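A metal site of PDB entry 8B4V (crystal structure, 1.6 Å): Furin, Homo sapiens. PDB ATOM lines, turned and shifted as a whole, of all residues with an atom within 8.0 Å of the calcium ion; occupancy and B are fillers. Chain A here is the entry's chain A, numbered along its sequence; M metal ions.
OD1 of Asp 8 is in hydrogen-bond range of N of Asn 100, 2.7 Å away.
A ring nitrogen (ND1) of His 53 lies within hydrogen-bond range of the backbone NH (N) of Asp 55, 3.0 Å away.
SG of Cys 253 is disulfide-bonded to SG of Cys 104, 2.0 Å away.
O of Val 103 binds the calcium ion, at 2.3 Å.
The calcium ion is bound by O of Val 98, at 2.3 Å.
The calcium ion is bound by OD2 of Asp 8 (2.4 Å).
OD1 of Asp 55 binds the calcium ion.
O of Gly 105 binds the calcium ion, at 2.4 Å.
The calcium ion is bound by OD1 of Asn 101 (2.5 Å).
The calcium ion is bound by OD2 of Asp 55 (2.6 Å).
The calcium ion has seven donor atoms within binding distance.
Six residues have an atom within 4 Å of the calcium ion: Asp 8, Asp 55, Val 98, Asn 101, Val 103 and Gly 105.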
ATOM      1  N   PRO A   6      23.913 -23.723 -20.281  1.00  0.00           N
ATOM      2  CA  PRO A   6      24.718 -23.095 -21.343  1.00  0.00           C
ATOM      3  C   PRO A   6      25.769 -24.015 -21.923  1.00  0.00           C
ATOM      4  O   PRO A   6      26.361 -24.852 -21.231  1.00  0.00           O
ATOM      5  CB  PRO A   6      25.360 -21.899 -20.617  1.00  0.00           C
ATOM      6  CG  PRO A   6      24.393 -21.572 -19.502  1.00  0.00           C
ATOM      7  CD  PRO A   6      23.901 -22.930 -19.043  1.00  0.00           C
ATOM      8  N   THR A   7      26.029 -23.831 -23.210  1.00  0.00           N
ATOM      9  CA  THR A   7      27.014 -24.589 -23.950  1.00  0.00           C
ATOM     10  C   THR A   7      28.345 -23.856 -24.083  1.00  0.00           C
ATOM     11  O   THR A   7      29.257 -24.373 -24.742  1.00  0.00           O
ATOM     12  CB  THR A   7      26.461 -24.930 -25.340  1.00  0.00           C
ATOM     13  OG1 THR A   7      26.126 -23.713 -26.019  1.00  0.00           O
ATOM     14  CG2 THR A   7      25.209 -25.795 -25.221  1.00  0.00           C
ATOM     15  N   ASP A   8      28.485 -22.684 -23.471  1.00  0.00           N
ATOM     16  CA  ASP A   8      29.680 -21.879 -23.650  1.00  0.00           C
ATOM     17  C   ASP A   8      30.925 -22.649 -23.231  1.00  0.00           C
ATOM     18  O   ASP A   8      30.889 -23.461 -22.295  1.00  0.00           O
ATOM     19  CB  ASP A   8      29.554 -20.591 -22.856  1.00  0.00           C
ATOM     20  CG  ASP A   8      28.305 -19.816 -23.202  1.00  0.00           C
ATOM     21  OD1 ASP A   8      27.193 -20.353 -22.994  1.00  0.00           O
ATOM     22  OD2 ASP A   8      28.430 -18.671 -23.698  1.00  0.00           O
ATOM     23  N   PRO A   9      32.061 -22.398 -23.894  1.00  0.00           N
ATOM     24  CA  PRO A   9      33.247 -23.255 -23.704  1.00  0.00           C
ATOM     25  C   PRO A   9      33.802 -23.244 -22.295  1.00  0.00           C
ATOM     26  O   PRO A   9      34.307 -24.280 -21.837  1.00  0.00           O
ATOM     27  CB  PRO A   9      34.259 -22.698 -24.712  1.00  0.00           C
ATOM     28  CG  PRO A   9      33.762 -21.293 -25.046  1.00  0.00           C
ATOM     29  CD  PRO A   9      32.264 -21.391 -24.955  1.00  0.00           C
ATOM     30  N   LYS A  10      33.734 -22.107 -21.596  1.00  0.00           N
ATOM     31  CA  LYS A  10      34.239 -21.998 -20.230  1.00  0.00           C
ATOM     32  C   LYS A  10      33.143 -22.157 -19.172  1.00  0.00           C
ATOM     33  O   LYS A  10      33.440 -22.010 -17.987  1.00  0.00           O
ATOM     34  CB  LYS A  10      34.947 -20.650 -20.037  1.00  0.00           C
ATOM     35  CG  LYS A  10      36.209 -20.462 -20.896  1.00  0.00           C
ATOM     36  CD  LYS A  10      37.304 -21.447 -20.498  1.00  0.00           C
ATOM     37  CE  LYS A  10      38.473 -21.430 -21.478  1.00  0.00           C
ATOM     38  NZ  LYS A  10      39.365 -22.609 -21.262  1.00  0.00           N
ATOM     39  N   PHE A  11      31.905 -22.442 -19.568  1.00  0.00           N
ATOM     40  CA  PHE A  11      30.883 -22.651 -18.554  1.00  0.00           C
ATOM     41  C   PHE A  11      31.256 -23.771 -17.587  1.00  0.00           C
ATOM     42  O   PHE A  11      31.030 -23.609 -16.380  1.00  0.00           O
ATOM     43  CB  PHE A  11      29.507 -22.932 -19.187  1.00  0.00           C
ATOM     44  CG  PHE A  11      28.433 -23.206 -18.162  1.00  0.00           C
ATOM     45  CD1 PHE A  11      28.017 -22.222 -17.296  1.00  0.00           C
ATOM     46  CD2 PHE A  11      27.872 -24.479 -18.048  1.00  0.00           C
ATOM     47  CE1 PHE A  11      27.050 -22.476 -16.339  1.00  0.00           C
ATOM     48  CE2 PHE A  11      26.900 -24.728 -17.097  1.00  0.00           C
ATOM     49  CZ  PHE A  11      26.491 -23.735 -16.244  1.00  0.00           C
ATOM     50  N   GLN A  14      33.076 -22.490 -14.649  1.00  0.00           N
ATOM     51  CA  GLN A  14      32.364 -21.576 -13.739  1.00  0.00           C
ATOM     52  C   GLN A  14      31.753 -22.393 -12.599  1.00  0.00           C
ATOM     53  O   GLN A  14      30.537 -22.563 -12.468  1.00  0.00           O
ATOM     54  CB  GLN A  14      31.326 -20.779 -14.525  1.00  0.00           C
ATOM     55  CG  GLN A  14      32.003 -19.890 -15.553  1.00  0.00           C
ATOM     56  CD  GLN A  14      31.066 -18.975 -16.291  1.00  0.00           C
ATOM     57  OE1 GLN A  14      30.211 -19.422 -17.041  1.00  0.00           O
ATOM     58  NE2 GLN A  14      31.246 -17.674 -16.102  1.00  0.00           N
ATOM     59  N   HIS A  53      32.970  -6.015 -26.568  1.00  0.00           N
ATOM     60  CA  HIS A  53      33.468  -7.345 -26.257  1.00  0.00           C
ATOM     61  C   HIS A  53      32.523  -8.395 -26.840  1.00  0.00           C
ATOM     62  O   HIS A  53      31.304  -8.246 -26.736  1.00  0.00           O
ATOM     63  CB  HIS A  53      33.615  -7.530 -24.740  1.00  0.00           C
ATOM     64  CG  HIS A  53      34.414  -8.730 -24.356  1.00  0.00           C
ATOM     65  ND1 HIS A  53      33.994 -10.022 -24.631  1.00  0.00           N
ATOM     66  CD2 HIS A  53      35.616  -8.854 -23.747  1.00  0.00           C
ATOM     67  CE1 HIS A  53      34.899 -10.880 -24.213  1.00  0.00           C
ATOM     68  NE2 HIS A  53      35.896 -10.201 -23.662  1.00  0.00           N
ATOM     69  N   PRO A  54      33.039  -9.444 -27.479  1.00  0.00           N
ATOM     70  CA  PRO A  54      32.134 -10.426 -28.108  1.00  0.00           C
ATOM     71  C   PRO A  54      31.185 -11.099 -27.118  1.00  0.00           C
ATOM     72  O   PRO A  54      30.127 -11.584 -27.545  1.00  0.00           O
ATOM     73  CB  PRO A  54      33.080 -11.444 -28.761  1.00  0.00           C
ATOM     74  CG  PRO A  54      34.463 -11.098 -28.312  1.00  0.00           C
ATOM     75  CD  PRO A  54      34.457  -9.680 -27.811  1.00  0.00           C
ATOM     76  N   ASP A  55      31.497 -11.139 -25.834  1.00  0.00           N
ATOM     77  CA  ASP A  55      30.579 -11.725 -24.866  1.00  0.00           C
ATOM     78  C   ASP A  55      29.773 -10.682 -24.093  1.00  0.00           C
ATOM     79  O   ASP A  55      29.014 -11.062 -23.184  1.00  0.00           O
ATOM     80  CB  ASP A  55      31.335 -12.629 -23.890  1.00  0.00           C
ATOM     81  CG  ASP A  55      30.652 -13.982 -23.689  1.00  0.00           C
ATOM     82  OD1 ASP A  55      29.862 -14.414 -24.572  1.00  0.00           O
ATOM     83  OD2 ASP A  55      30.901 -14.625 -22.646  1.00  0.00           O
ATOM     84  N   LEU A  56      29.889  -9.387 -24.420  1.00  0.00           N
ATOM     85  CA  LEU A  56      29.061  -8.351 -23.813  1.00  0.00           C
ATOM     86  C   LEU A  56      28.182  -7.594 -24.799  1.00  0.00           C
ATOM     87  O   LEU A  56      27.112  -7.117 -24.405  1.00  0.00           O
ATOM     88  CB  LEU A  56      29.924  -7.318 -23.069  1.00  0.00           C
ATOM     89  CG  LEU A  56      30.831  -7.830 -21.951  1.00  0.00           C
ATOM     90  CD1 LEU A  56      31.713  -6.718 -21.452  1.00  0.00           C
ATOM     91  CD2 LEU A  56      30.011  -8.410 -20.831  1.00  0.00           C
ATOM     92  N   GLY A  93      31.058  -8.944 -17.181  1.00  0.00           N
ATOM     93  CA  GLY A  93      30.818 -10.294 -17.657  1.00  0.00           C
ATOM     94  C   GLY A  93      30.310 -11.229 -16.586  1.00  0.00           C
ATOM     95  O   GLY A  93      29.606 -12.197 -16.882  1.00  0.00           O
ATOM     96  N   ALA A  96      26.509 -10.400 -16.708  1.00  0.00           N
ATOM     97  CA  ALA A  96      25.669 -10.507 -17.897  1.00  0.00           C
ATOM     98  C   ALA A  96      26.420 -10.892 -19.165  1.00  0.00           C
ATOM     99  O   ALA A  96      26.003 -10.498 -20.264  1.00  0.00           O
ATOM    100  CB  ALA A  96      24.938  -9.183 -18.152  1.00  0.00           C
ATOM    101  N   ALA A  97      27.496 -11.654 -19.068  1.00  0.00           N
ATOM    102  CA  ALA A  97      28.080 -12.223 -20.281  1.00  0.00           C
ATOM    103  C   ALA A  97      27.029 -13.041 -21.035  1.00  0.00           C
ATOM    104  O   ALA A  97      26.233 -13.771 -20.433  1.00  0.00           O
ATOM    105  CB  ALA A  97      29.296 -13.102 -19.959  1.00  0.00           C
ATOM    106  N   VAL A  98      27.034 -12.908 -22.374  1.00  0.00           N
ATOM    107  CA  VAL A  98      26.070 -13.601 -23.207  1.00  0.00           C
ATOM    108  C   VAL A  98      26.267 -15.106 -23.126  1.00  0.00           C
ATOM    109  O   VAL A  98      27.388 -15.620 -23.003  1.00  0.00           O
ATOM    110  CB  VAL A  98      26.233 -13.110 -24.667  1.00  0.00           C
ATOM    111  CG1 VAL A  98      25.356 -13.907 -25.638  1.00  0.00           C
ATOM    112  CG2 VAL A  98      25.904 -11.629 -24.759  1.00  0.00           C
ATOM    113  N   ALA A  99      25.154 -15.836 -23.200  1.00  0.00           N
ATOM    114  CA  ALA A  99      25.155 -17.289 -23.119  1.00  0.00           C
ATOM    115  C   ALA A  99      24.937 -17.921 -24.482  1.00  0.00           C
ATOM    116  O   ALA A  99      24.313 -17.342 -25.381  1.00  0.00           O
ATOM    117  CB  ALA A  99      24.053 -17.777 -22.164  1.00  0.00           C
ATOM    118  N   ASN A 100      25.445 -19.158 -24.622  1.00  0.00           N
ATOM    119  CA  ASN A 100      25.185 -20.023 -25.773  1.00  0.00           C
ATOM    120  C   ASN A 100      25.658 -19.396 -27.080  1.00  0.00           C
ATOM    121  O   ASN A 100      25.035 -19.555 -28.126  1.00  0.00           O
ATOM    122  CB  ASN A 100      23.696 -20.384 -25.846  1.00  0.00           C
ATOM    123  CG  ASN A 100      23.239 -21.194 -24.646  1.00  0.00           C
ATOM    124  OD1 ASN A 100      23.816 -22.235 -24.331  1.00  0.00           O
ATOM    125  ND2 ASN A 100      22.218 -20.702 -23.956  1.00  0.00           N
ATOM    126  N   ASN A 101      26.798 -18.718 -27.015  1.00  0.00           N
ATOM    127  CA  ASN A 101      27.371 -18.031 -28.169  1.00  0.00           C
ATOM    128  C   ASN A 101      28.807 -18.460 -28.461  1.00  0.00           C
ATOM    129  O   ASN A 101      29.491 -17.789 -29.237  1.00  0.00           O
ATOM    130  CB  ASN A 101      27.287 -16.516 -27.961  1.00  0.00           C
ATOM    131  CG  ASN A 101      28.262 -16.012 -26.901  1.00  0.00           C
ATOM    132  OD1 ASN A 101      28.676 -16.739 -25.992  1.00  0.00           O
ATOM    133  ND2 ASN A 101      28.629 -14.744 -27.024  1.00  0.00           N
ATOM    134  N   GLY A 102      29.269 -19.562 -27.870  1.00  0.00           N
ATOM    135  CA  GLY A 102      30.587 -20.071 -28.174  1.00  0.00           C
ATOM    136  C   GLY A 102      31.751 -19.251 -27.671  1.00  0.00           C
ATOM    137  O   GLY A 102      32.889 -19.508 -28.086  1.00  0.00           O
ATOM    138  N   VAL A 103      31.508 -18.285 -26.786  1.00  0.00           N
ATOM    139  CA  VAL A 103      32.537 -17.390 -26.278  1.00  0.00           C
ATOM    140  C   VAL A 103      32.556 -17.464 -24.757  1.00  0.00           C
ATOM    141  O   VAL A 103      31.509 -17.362 -24.116  1.00  0.00           O
ATOM    142  CB  VAL A 103      32.296 -15.934 -26.739  1.00  0.00           C
ATOM    143  CG1 VAL A 103      33.325 -14.985 -26.130  1.00  0.00           C
ATOM    144  CG2 VAL A 103      32.314 -15.853 -28.266  1.00  0.00           C
ATOM    145  N   CYS A 104      33.745 -17.668 -24.182  1.00  0.00           N
ATOM    146  CA  CYS A 104      34.023 -17.603 -22.738  1.00  0.00           C
ATOM    147  C   CYS A 104      32.922 -18.330 -21.965  1.00  0.00           C
ATOM    148  O   CYS A 104      32.633 -19.486 -22.297  1.00  0.00           O
ATOM    149  CB  CYS A 104      34.223 -16.126 -22.362  1.00  0.00           C
ATOM    150  SG  CYS A 104      35.108 -15.771 -20.811  1.00  0.00           S
ATOM    151  N   GLY A 105      32.356 -17.736 -20.920  1.00  0.00           N
ATOM    152  CA  GLY A 105      31.335 -18.402 -20.137  1.00  0.00           C
ATOM    153  C   GLY A 105      30.033 -17.626 -20.183  1.00  0.00           C
ATOM    154  O   GLY A 105      29.680 -17.088 -21.244  1.00  0.00           O
ATOM    155  N   VAL A 106      29.316 -17.532 -19.061  1.00  0.00           N
ATOM    156  CA  VAL A 106      28.039 -16.833 -19.041  1.00  0.00           C
ATOM    157  C   VAL A 106      27.980 -15.933 -17.822  1.00  0.00           C
ATOM    158  O   VAL A 106      28.641 -16.172 -16.804  1.00  0.00           O
ATOM    159  CB  VAL A 106      26.817 -17.792 -19.037  1.00  0.00           C
ATOM    160  CG1 VAL A 106      26.872 -18.768 -20.197  1.00  0.00           C
ATOM    161  CG2 VAL A 106      26.704 -18.509 -17.707  1.00  0.00           C
ATOM    162  N   GLY A 107      27.143 -14.899 -17.917  1.00  0.00           N
ATOM    163  CA  GLY A 107      26.782 -14.131 -16.756  1.00  0.00           C
ATOM    164  C   GLY A 107      25.754 -14.847 -15.889  1.00  0.00           C
ATOM    165  O   GLY A 107      25.037 -15.733 -16.336  1.00  0.00           O
ATOM    166  N   TYR A 110      22.333 -13.808 -17.644  1.00  0.00           N
ATOM    167  CA  TYR A 110      22.883 -13.743 -18.991  1.00  0.00           C
ATOM    168  C   TYR A 110      21.912 -13.197 -20.025  1.00  0.00           C
ATOM    169  O   TYR A 110      22.316 -13.047 -21.188  1.00  0.00           O
ATOM    170  CB  TYR A 110      23.411 -15.119 -19.426  1.00  0.00           C
ATOM    171  CG  TYR A 110      22.470 -16.305 -19.385  1.00  0.00           C
ATOM    172  CD1 TYR A 110      21.438 -16.439 -20.300  1.00  0.00           C
ATOM    173  CD2 TYR A 110      22.690 -17.347 -18.492  1.00  0.00           C
ATOM    174  CE1 TYR A 110      20.613 -17.549 -20.297  1.00  0.00           C
ATOM    175  CE2 TYR A 110      21.868 -18.475 -18.478  1.00  0.00           C
ATOM    176  CZ  TYR A 110      20.832 -18.562 -19.392  1.00  0.00           C
ATOM    177  OH  TYR A 110      20.002 -19.666 -19.395  1.00  0.00           O
ATOM    178  N   THR A 247      34.730 -12.140 -18.780  1.00  0.00           N
ATOM    179  CA  THR A 247      35.226 -11.354 -19.905  1.00  0.00           C
ATOM    180  C   THR A 247      36.388 -10.463 -19.476  1.00  0.00           C
ATOM    181  O   THR A 247      36.378  -9.870 -18.399  1.00  0.00           O
ATOM    182  CB  THR A 247      34.089 -10.474 -20.435  1.00  0.00           C
ATOM    183  OG1 THR A 247      33.447  -9.814 -19.343  1.00  0.00           O
ATOM    184  CG2 THR A 247      33.069 -11.315 -21.155  1.00  0.00           C
ATOM    185  N   CYS A 253      39.158 -13.718 -22.522  1.00  0.00           N
ATOM    186  CA  CYS A 253      38.457 -14.460 -21.478  1.00  0.00           C
ATOM    187  C   CYS A 253      39.451 -14.826 -20.386  1.00  0.00           C
ATOM    188  O   CYS A 253      40.454 -15.483 -20.659  1.00  0.00           O
ATOM    189  CB  CYS A 253      37.829 -15.732 -22.080  1.00  0.00           C
ATOM    190  SG  CYS A 253      36.874 -16.771 -20.971  1.00  0.00           S
HETATM  191 CA    CA M   1      29.434 -16.530 -23.576  1.00  0.00          CA
